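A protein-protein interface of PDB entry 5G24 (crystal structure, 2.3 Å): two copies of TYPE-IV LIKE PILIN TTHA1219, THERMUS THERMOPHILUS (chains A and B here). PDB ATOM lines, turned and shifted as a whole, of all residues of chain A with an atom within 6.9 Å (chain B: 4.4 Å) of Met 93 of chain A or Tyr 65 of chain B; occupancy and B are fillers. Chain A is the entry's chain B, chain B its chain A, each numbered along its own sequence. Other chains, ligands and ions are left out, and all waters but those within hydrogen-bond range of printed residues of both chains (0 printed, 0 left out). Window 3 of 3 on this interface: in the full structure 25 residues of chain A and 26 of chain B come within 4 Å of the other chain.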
ATOM      1  N   ARG A  58     -23.339  -3.842 -25.167  1.00  0.00           N
ATOM      2  CA  ARG A  58     -23.534  -5.184 -24.553  1.00  0.00           C
ATOM      3  C   ARG A  58     -24.897  -5.334 -23.868  1.00  0.00           C
ATOM      4  O   ARG A  58     -25.551  -6.353 -23.990  1.00  0.00           O
ATOM      5  CB  ARG A  58     -22.442  -5.482 -23.543  1.00  0.00           C
ATOM      6  CG  ARG A  58     -22.317  -6.964 -23.348  1.00  0.00           C
ATOM      7  CD  ARG A  58     -21.546  -7.365 -22.075  1.00  0.00           C
ATOM      8  NE  ARG A  58     -21.291  -8.832 -22.035  1.00  0.00           N
ATOM      9  CZ  ARG A  58     -20.109  -9.437 -22.193  1.00  0.00           C
ATOM     10  NH1 ARG A  58     -18.975  -8.730 -22.398  1.00  0.00           N
ATOM     11  NH2 ARG A  58     -20.052 -10.781 -22.106  1.00  0.00           N
ATOM     12  N   THR A  62     -28.808  -7.535 -25.847  1.00  0.00           N
ATOM     13  CA  THR A  62     -29.651  -8.529 -25.203  1.00  0.00           C
ATOM     14  C   THR A  62     -31.176  -8.167 -25.132  1.00  0.00           C
ATOM     15  O   THR A  62     -31.972  -9.074 -24.884  1.00  0.00           O
ATOM     16  CB  THR A  62     -29.252  -8.788 -23.758  1.00  0.00           C
ATOM     17  OG1 THR A  62     -29.463  -7.575 -23.021  1.00  0.00           O
ATOM     18  CG2 THR A  62     -27.760  -9.211 -23.646  1.00  0.00           C
ATOM     19  N   TYR A  65     -34.348 -10.557 -25.410  1.00  0.00           N
ATOM     20  CA  TYR A  65     -33.950 -11.979 -25.270  1.00  0.00           C
ATOM     21  C   TYR A  65     -35.021 -12.828 -24.584  1.00  0.00           C
ATOM     22  O   TYR A  65     -35.374 -12.631 -23.407  1.00  0.00           O
ATOM     23  CB  TYR A  65     -32.608 -12.126 -24.498  1.00  0.00           C
ATOM     24  CG  TYR A  65     -32.075 -13.557 -24.489  1.00  0.00           C
ATOM     25  CD1 TYR A  65     -31.445 -14.089 -25.611  1.00  0.00           C
ATOM     26  CD2 TYR A  65     -32.219 -14.382 -23.357  1.00  0.00           C
ATOM     27  CE1 TYR A  65     -30.981 -15.420 -25.610  1.00  0.00           C
ATOM     28  CE2 TYR A  65     -31.795 -15.734 -23.357  1.00  0.00           C
ATOM     29  CZ  TYR A  65     -31.174 -16.239 -24.488  1.00  0.00           C
ATOM     30  OH  TYR A  65     -30.720 -17.540 -24.517  1.00  0.00           O
ATOM     31  N   PHE A  87     -35.631  -7.828 -21.028  1.00  0.00           N
ATOM     32  CA  PHE A  87     -35.132  -9.118 -21.477  1.00  0.00           C
ATOM     33  C   PHE A  87     -35.276 -10.183 -20.419  1.00  0.00           C
ATOM     34  O   PHE A  87     -35.434  -9.890 -19.230  1.00  0.00           O
ATOM     35  CB  PHE A  87     -33.671  -9.004 -21.912  1.00  0.00           C
ATOM     36  CG  PHE A  87     -32.746  -8.514 -20.838  1.00  0.00           C
ATOM     37  CD1 PHE A  87     -32.185  -9.409 -19.935  1.00  0.00           C
ATOM     38  CD2 PHE A  87     -32.410  -7.185 -20.724  1.00  0.00           C
ATOM     39  CE1 PHE A  87     -31.302  -9.006 -18.902  1.00  0.00           C
ATOM     40  CE2 PHE A  87     -31.508  -6.758 -19.714  1.00  0.00           C
ATOM     41  CZ  PHE A  87     -30.980  -7.683 -18.773  1.00  0.00           C
ATOM     42  N   LEU A  88     -35.263 -11.429 -20.854  1.00  0.00           N
ATOM     43  CA  LEU A  88     -35.361 -12.568 -19.921  1.00  0.00           C
ATOM     44  C   LEU A  88     -33.974 -12.972 -19.436  1.00  0.00           C
ATOM     45  O   LEU A  88     -33.072 -13.125 -20.246  1.00  0.00           O
ATOM     46  CB  LEU A  88     -36.020 -13.782 -20.569  1.00  0.00           C
ATOM     47  CG  LEU A  88     -36.441 -14.928 -19.601  1.00  0.00           C
ATOM     48  CD1 LEU A  88     -37.650 -14.546 -18.741  1.00  0.00           C
ATOM     49  CD2 LEU A  88     -36.727 -16.220 -20.367  1.00  0.00           C
ATOM     50  N   CYS A  89     -33.812 -13.082 -18.119  1.00  0.00           N
ATOM     51  CA  CYS A  89     -32.603 -13.627 -17.511  1.00  0.00           C
ATOM     52  C   CYS A  89     -32.580 -15.144 -17.543  1.00  0.00           C
ATOM     53  O   CYS A  89     -33.417 -15.793 -16.949  1.00  0.00           O
ATOM     54  CB  CYS A  89     -32.453 -13.164 -16.058  1.00  0.00           C
ATOM     55  SG  CYS A  89     -31.744 -11.533 -15.999  1.00  0.00           S
ATOM     56  N   GLU A  90     -31.590 -15.680 -18.235  1.00  0.00           N
ATOM     57  CA  GLU A  90     -31.058 -17.017 -17.952  1.00  0.00           C
ATOM     58  C   GLU A  90     -29.758 -16.825 -17.157  1.00  0.00           C
ATOM     59  O   GLU A  90     -28.761 -16.301 -17.694  1.00  0.00           O
ATOM     60  CB  GLU A  90     -30.731 -17.765 -19.232  1.00  0.00           C
ATOM     61  CG  GLU A  90     -31.941 -18.223 -20.039  1.00  0.00           C
ATOM     62  CD  GLU A  90     -31.554 -18.864 -21.375  1.00  0.00           C
ATOM     63  OE1 GLU A  90     -30.364 -19.171 -21.573  1.00  0.00           O
ATOM     64  OE2 GLU A  90     -32.435 -19.039 -22.251  1.00  0.00           O
ATOM     65  N   ALA A  91     -29.777 -17.209 -15.877  1.00  0.00           N
ATOM     66  CA  ALA A  91     -28.584 -17.048 -15.002  1.00  0.00           C
ATOM     67  C   ALA A  91     -27.425 -17.865 -15.615  1.00  0.00           C
ATOM     68  O   ALA A  91     -27.644 -18.952 -16.132  1.00  0.00           O
ATOM     69  CB  ALA A  91     -28.870 -17.477 -13.553  1.00  0.00           C
ATOM     70  N   GLY A  92     -26.227 -17.280 -15.629  1.00  0.00           N
ATOM     71  CA  GLY A  92     -25.000 -17.898 -16.218  1.00  0.00           C
ATOM     72  C   GLY A  92     -24.390 -17.176 -17.447  1.00  0.00           C
ATOM     73  O   GLY A  92     -23.182 -17.291 -17.735  1.00  0.00           O
ATOM     74  N   MET A  93     -25.226 -16.443 -18.179  1.00  0.00           N
ATOM     75  CA  MET A  93     -24.822 -15.884 -19.483  1.00  0.00           C
ATOM     76  C   MET A  93     -24.552 -14.355 -19.447  1.00  0.00           C
ATOM     77  O   MET A  93     -23.715 -13.870 -20.214  1.00  0.00           O
ATOM     78  CB  MET A  93     -25.798 -16.321 -20.628  1.00  0.00           C
ATOM     79  CG  MET A  93     -27.267 -15.874 -20.539  1.00  0.00           C
ATOM     80  SD  MET A  93     -28.166 -15.777 -22.128  1.00  0.00           S
ATOM     81  CE  MET A  93     -27.908 -14.025 -22.649  1.00  0.00           C
ATOM     82  N   GLU A  94     -25.243 -13.618 -18.564  1.00  0.00           N
ATOM     83  CA  GLU A  94     -25.119 -12.155 -18.435  1.00  0.00           C
ATOM     84  C   GLU A  94     -25.169 -11.782 -16.977  1.00  0.00           C
ATOM     85  O   GLU A  94     -25.890 -12.396 -16.172  1.00  0.00           O
ATOM     86  CB  GLU A  94     -26.174 -11.382 -19.237  1.00  0.00           C
ATOM     87  CG  GLU A  94     -26.031 -11.507 -20.796  1.00  0.00           C
ATOM     88  CD  GLU A  94     -24.711 -10.920 -21.448  1.00  0.00           C
ATOM     89  OE1 GLU A  94     -24.366  -9.708 -21.247  1.00  0.00           O
ATOM     90  OE2 GLU A  94     -23.996 -11.669 -22.208  1.00  0.00           O
ATOM     91  N   GLU A  95     -24.287 -10.833 -16.636  1.00  0.00           N
ATOM     92  CA  GLU A  95     -23.853 -10.628 -15.273  1.00  0.00           C
ATOM     93  C   GLU A  95     -25.001 -10.245 -14.323  1.00  0.00           C
ATOM     94  O   GLU A  95     -25.207 -10.885 -13.256  1.00  0.00           O
ATOM     95  CB  GLU A  95     -22.661  -9.636 -15.232  1.00  0.00           C
ATOM     96  CG  GLU A  95     -21.891  -9.736 -13.895  1.00  0.00           C
ATOM     97  CD  GLU A  95     -21.584  -8.450 -13.166  1.00  0.00           C
ATOM     98  OE1 GLU A  95     -21.754  -7.339 -13.771  1.00  0.00           O
ATOM     99  OE2 GLU A  95     -21.095  -8.600 -11.977  1.00  0.00           O
ATOM    100  N   CYS A  97     -27.985 -10.970 -14.172  1.00  0.00           N
ATOM    101  CA  CYS A  97     -28.762 -12.148 -13.817  1.00  0.00           C
ATOM    102  C   CYS A  97     -27.959 -13.071 -12.933  1.00  0.00           C
ATOM    103  O   CYS A  97     -28.415 -13.457 -11.865  1.00  0.00           O
ATOM    104  CB  CYS A  97     -29.165 -12.869 -15.120  1.00  0.00           C
ATOM    105  SG  CYS A  97     -29.769 -11.755 -16.487  1.00  0.00           S
ATOM    106  N   TYR B  61     -17.696 -12.639 -16.076  1.00  0.00           N
ATOM    107  CA  TYR B  61     -18.810 -13.371 -15.643  1.00  0.00           C
ATOM    108  C   TYR B  61     -19.112 -14.548 -16.581  1.00  0.00           C
ATOM    109  O   TYR B  61     -19.585 -15.584 -16.108  1.00  0.00           O
ATOM    110  CB  TYR B  61     -20.050 -12.496 -15.608  1.00  0.00           C
ATOM    111  CG  TYR B  61     -21.312 -13.189 -15.087  1.00  0.00           C
ATOM    112  CD1 TYR B  61     -21.568 -13.262 -13.716  1.00  0.00           C
ATOM    113  CD2 TYR B  61     -22.235 -13.744 -15.962  1.00  0.00           C
ATOM    114  CE1 TYR B  61     -22.699 -13.855 -13.238  1.00  0.00           C
ATOM    115  CE2 TYR B  61     -23.395 -14.379 -15.492  1.00  0.00           C
ATOM    116  CZ  TYR B  61     -23.628 -14.414 -14.123  1.00  0.00           C
ATOM    117  OH  TYR B  61     -24.793 -15.013 -13.616  1.00  0.00           O
ATOM    118  N   THR B  62     -18.880 -14.366 -17.879  1.00  0.00           N
ATOM    119  CA  THR B  62     -19.179 -15.409 -18.860  1.00  0.00           C
ATOM    120  C   THR B  62     -18.126 -16.523 -18.951  1.00  0.00           C
ATOM    121  O   THR B  62     -18.394 -17.573 -19.523  1.00  0.00           O
ATOM    122  CB  THR B  62     -19.306 -14.852 -20.290  1.00  0.00           C
ATOM    123  OG1 THR B  62     -18.034 -14.310 -20.635  1.00  0.00           O
ATOM    124  CG2 THR B  62     -20.391 -13.789 -20.390  1.00  0.00           C
ATOM    125  N   VAL B  63     -16.969 -16.321 -18.387  1.00  0.00           N
ATOM    126  CA  VAL B  63     -15.905 -17.237 -18.533  1.00  0.00           C
ATOM    127  C   VAL B  63     -16.359 -18.605 -18.070  1.00  0.00           C
ATOM    128  O   VAL B  63     -17.064 -18.751 -17.076  1.00  0.00           O
ATOM    129  CB  VAL B  63     -14.627 -16.688 -17.760  1.00  0.00           C
ATOM    130  CG1 VAL B  63     -13.624 -17.785 -17.481  1.00  0.00           C
ATOM    131  CG2 VAL B  63     -13.958 -15.572 -18.573  1.00  0.00           C
ATOM    132  N   GLY B  64     -15.956 -19.613 -18.818  1.00  0.00           N
ATOM    133  CA  GLY B  64     -16.409 -21.002 -18.598  1.00  0.00           C
ATOM    134  C   GLY B  64     -17.785 -21.368 -19.141  1.00  0.00           C
ATOM    135  O   GLY B  64     -18.199 -22.500 -19.003  1.00  0.00           O
ATOM    136  N   TYR B  65     -18.505 -20.420 -19.734  1.00  0.00           N
ATOM    137  CA  TYR B  65     -19.847 -20.697 -20.207  1.00  0.00           C
ATOM    138  C   TYR B  65     -19.846 -21.854 -21.220  1.00  0.00           C
ATOM    139  O   TYR B  65     -19.308 -21.764 -22.330  1.00  0.00           O
ATOM    140  CB  TYR B  65     -20.512 -19.468 -20.857  1.00  0.00           C
ATOM    141  CG  TYR B  65     -21.976 -19.679 -21.205  1.00  0.00           C
ATOM    142  CD1 TYR B  65     -22.981 -19.654 -20.217  1.00  0.00           C
ATOM    143  CD2 TYR B  65     -22.374 -19.900 -22.526  1.00  0.00           C
ATOM    144  CE1 TYR B  65     -24.337 -19.813 -20.546  1.00  0.00           C
ATOM    145  CE2 TYR B  65     -23.730 -20.062 -22.861  1.00  0.00           C
ATOM    146  CZ  TYR B  65     -24.702 -20.016 -21.876  1.00  0.00           C
ATOM    147  OH  TYR B  65     -25.997 -20.251 -22.162  1.00  0.00           O
ATOM    148  N   ARG B  66     -20.472 -22.939 -20.785  1.00  0.00           N
ATOM    149  CA  ARG B  66     -20.821 -24.062 -21.658  1.00  0.00           C
ATOM    150  C   ARG B  66     -19.545 -24.720 -22.245  1.00  0.00           C
ATOM    151  O   ARG B  66     -19.575 -25.338 -23.327  1.00  0.00           O
ATOM    152  CB  ARG B  66     -21.827 -23.593 -22.778  1.00  0.00           C
ATOM    153  CG  ARG B  66     -23.070 -24.394 -22.764  1.00  0.00           C
ATOM    154  CD  ARG B  66     -24.222 -23.918 -23.658  1.00  0.00           C
ATOM    155  NE  ARG B  66     -24.905 -25.107 -24.314  1.00  0.00           N
ATOM    156  CZ  ARG B  66     -26.175 -25.159 -24.756  1.00  0.00           C
ATOM    157  NH1 ARG B  66     -26.977 -24.079 -24.683  1.00  0.00           N
ATOM    158  NH2 ARG B  66     -26.665 -26.300 -25.294  1.00  0.00           N
ATOM    159  N   LEU B  67     -18.444 -24.570 -21.521  1.00  0.00           N
ATOM    160  CA  LEU B  67     -17.139 -24.977 -21.986  1.00  0.00           C
ATOM    161  C   LEU B  67     -16.710 -26.220 -21.242  1.00  0.00           C
ATOM    162  O   LEU B  67     -16.996 -26.363 -20.046  1.00  0.00           O
ATOM    163  CB  LEU B  67     -16.139 -23.872 -21.682  1.00  0.00           C
ATOM    164  CG  LEU B  67     -14.762 -23.976 -22.362  1.00  0.00           C
ATOM    165  CD1 LEU B  67     -14.763 -23.191 -23.663  1.00  0.00           C
ATOM    166  CD2 LEU B  67     -13.670 -23.423 -21.448  1.00  0.00           C
ATOM    167  N   PHE B  87     -14.646 -19.245 -23.182  1.00  0.00           N
ATOM    168  CA  PHE B  87     -16.079 -19.503 -23.074  1.00  0.00           C
ATOM    169  C   PHE B  87     -16.671 -19.956 -24.418  1.00  0.00           C
ATOM    170  O   PHE B  87     -16.112 -19.619 -25.476  1.00  0.00           O
ATOM    171  CB  PHE B  87     -16.837 -18.315 -22.483  1.00  0.00           C
ATOM    172  CG  PHE B  87     -16.776 -17.052 -23.300  1.00  0.00           C
ATOM    173  CD1 PHE B  87     -15.680 -16.203 -23.220  1.00  0.00           C
ATOM    174  CD2 PHE B  87     -17.820 -16.706 -24.183  1.00  0.00           C
ATOM    175  CE1 PHE B  87     -15.600 -15.042 -23.974  1.00  0.00           C
ATOM    176  CE2 PHE B  87     -17.758 -15.536 -24.951  1.00  0.00           C
ATOM    177  CZ  PHE B  87     -16.637 -14.708 -24.841  1.00  0.00           C
ATOM    178  N   LEU B  88     -17.809 -20.657 -24.370  1.00  0.00           N
ATOM    179  CA  LEU B  88     -18.557 -20.961 -25.593  1.00  0.00           C
ATOM    180  C   LEU B  88     -19.453 -19.783 -26.014  1.00  0.00           C
ATOM    181  O   LEU B  88     -20.211 -19.259 -25.215  1.00  0.00           O
ATOM    182  CB  LEU B  88     -19.406 -22.216 -25.407  1.00  0.00           C
ATOM    183  CG  LEU B  88     -19.930 -22.866 -26.688  1.00  0.00           C
ATOM    184  CD1 LEU B  88     -18.804 -23.514 -27.517  1.00  0.00           C
ATOM    185  CD2 LEU B  88     -21.032 -23.892 -26.410  1.00  0.00           C
ATOM    186  N   GLU B  90     -22.720 -18.799 -27.777  1.00  0.00           N
ATOM    187  CA  GLU B  90     -24.039 -19.029 -28.393  1.00  0.00           C
ATOM    188  C   GLU B  90     -24.400 -17.747 -29.112  1.00  0.00           C
ATOM    189  O   GLU B  90     -24.594 -16.716 -28.442  1.00  0.00           O
ATOM    190  CB  GLU B  90     -25.094 -19.338 -27.326  1.00  0.00           C
ATOM    191  CG  GLU B  90     -25.014 -20.739 -26.736  1.00  0.00           C
ATOM    192  CD  GLU B  90     -25.991 -20.956 -25.587  1.00  0.00           C
ATOM    193  OE1 GLU B  90     -26.921 -20.140 -25.422  1.00  0.00           O
ATOM    194  OE2 GLU B  90     -25.848 -21.955 -24.847  1.00  0.00           O
ATOM    195  N   MET B  93     -26.288 -14.249 -27.772  1.00  0.00           N
ATOM    196  CA  MET B  93     -25.958 -13.805 -26.381  1.00  0.00           C
ATOM    197  C   MET B  93     -25.045 -12.570 -26.313  1.00  0.00           C
ATOM    198  O   MET B  93     -25.230 -11.720 -25.438  1.00  0.00           O
ATOM    199  CB  MET B  93     -25.380 -14.978 -25.553  1.00  0.00           C
ATOM    200  CG  MET B  93     -23.863 -15.279 -25.625  1.00  0.00           C
ATOM    201  SD  MET B  93     -23.215 -16.570 -24.471  1.00  0.00           S
ATOM    202  CE  MET B  93     -22.729 -15.626 -22.990  1.00  0.00           C
ATOM    203  N   ASN B 233     -20.210 -19.961 -13.749  1.00  0.00           N
ATOM    204  CA  ASN B 233     -19.769 -21.011 -14.718  1.00  0.00           C
ATOM    205  C   ASN B 233     -18.552 -21.779 -14.269  1.00  0.00           C
ATOM    206  O   ASN B 233     -18.388 -22.897 -14.694  1.00  0.00           O
ATOM    207  CB  ASN B 233     -19.463 -20.424 -16.113  1.00  0.00           C
ATOM    208  CG  ASN B 233     -20.668 -19.743 -16.757  1.00  0.00           C
ATOM    209  OD1 ASN B 233     -21.716 -20.346 -16.880  1.00  0.00           O
ATOM    210  ND2 ASN B 233     -20.506 -18.502 -17.180  1.00  0.00           N
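The backbone carbonyl oxygen (O) of Thr 62 of chain B sits at hydrogen-bond distance from the side-chain amide nitrogen (ND2) of Asn 233 of chain B, at 3.3 Å. NE of Arg 58 of chain A is in salt-bridge range of OE1 of Glu 94 of chain A. The side-chain amide nitrogen (ND2) of Asn 233 of chain B lies close to the backbone carbonyl oxygen (O) of Val 63 of chain B, 3.5 Å away. OH of Tyr 65 of chain B sits at hydrogen-bond distance from OE2 of Glu 90 of chain B (3.2 Å). The side-chain amide nitrogen (ND2) of Asn 233 of chain B sits at hydrogen-bond distance from the backbone carbonyl oxygen (O) of Tyr 61 of chain B. SG of Cys 97 of chain A is disulfide-bonded to SG of Cys 89 of chain A (2.0 Å).
Printed residues of chain A that touch a printed residue of chain B: Arg 58, Thr 62, Gly 92, Met 93, Glu 94, Glu 95 and Cys 97. Hydrophobic or aromatic side chains of chain A within 4 Å of the printed part of chain B: Met 93. Among the printed residues, no Asp or Glu carboxylate lies within 4 Å of a Lys or Arg side-chain nitrogen of the other chain.
Of the printed residues of chain B, Met 93 of chain A touches Tyr 61, Thr 62, Tyr 65 and Met 93. Printed residues of chain B within 4 Å of Glu 95 of chain A: Tyr 61 (3.5 Å). Of the printed residues of chain A, Tyr 61 of chain B touches Gly 92, Met 93, Glu 94, Glu 95 and Cys 97. Of the printed residues of chain A, Met 93 of chain B touches Thr 62, Met 93 and Glu 94. Of the printed residues of chain A, Asn 233 of chain B touches Gly 92. The nearest printed residue of chain B that does not touch Met 93 of chain A is Asn 233 of chain B (5.2 Å). The nearest residue of chain A that does not touch Tyr 65 of chain B is Glu 90 of chain A (4.5 Å). The nearest printed residue of chain B that does not touch Glu 95 of chain A is Thr 62 of chain B (6.2 Å).
Thr 62 of chain A touches Met 93 of chain B, and with the chains exchanged Met 93 of chain A touches Thr 62 of chain B. Met 93 of chain A touches Tyr 65 of chain B, but with the chains exchanged Tyr 65 of chain A does not touch Met 93 of chain B (5.3 Å). Met 93 of chain B touches its own counterpart, Met 93 of chain A. Positions printed for both chains: 62, 65, 87, 88, 90 and 93. Of the 13 pairs that touch across the chains among the printed residues, 3 have their exchanged pair printed and touching as well.
Among the printed residues, merely in contact across the chains: Arg 58 of chain A with Thr 62 of chain B (3.5 Å), Thr 62 of chain A with Met 93 of chain B (3.99 Å), Gly 92 of chain A with Tyr 65 of chain B (3.4 Å), Met 93 of chain A with Tyr 61 of chain B (3.9 Å), Met 93 of chain A with Thr 62 of chain B (3.3 Å), Met 93 of chain A with Tyr 65 of chain B (3.8 Å), Met 93 of chain A with Met 93 of chain B (3.4 Å), Glu 94 of chain A with Tyr 61 of chain B (3.3 Å), Glu 95 of chain A with Tyr 61 of chain B (3.5 Å) and Cys 97 of chain A with Tyr 61 of chain B (3.8 Å).
The side-chain hydroxyl (OH) of Tyr 61 of chain B sits at hydrogen-bond distance from the backbone NH (N) of Gly 92 of chain A. OE2 of Glu 94 of chain A sits close to O of Met 93 of chain B, at 3.5 Å. ND2 of Asn 233 of chain B sits at hydrogen-bond distance from O of Gly 92 of chain A, at 3.0 Å.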
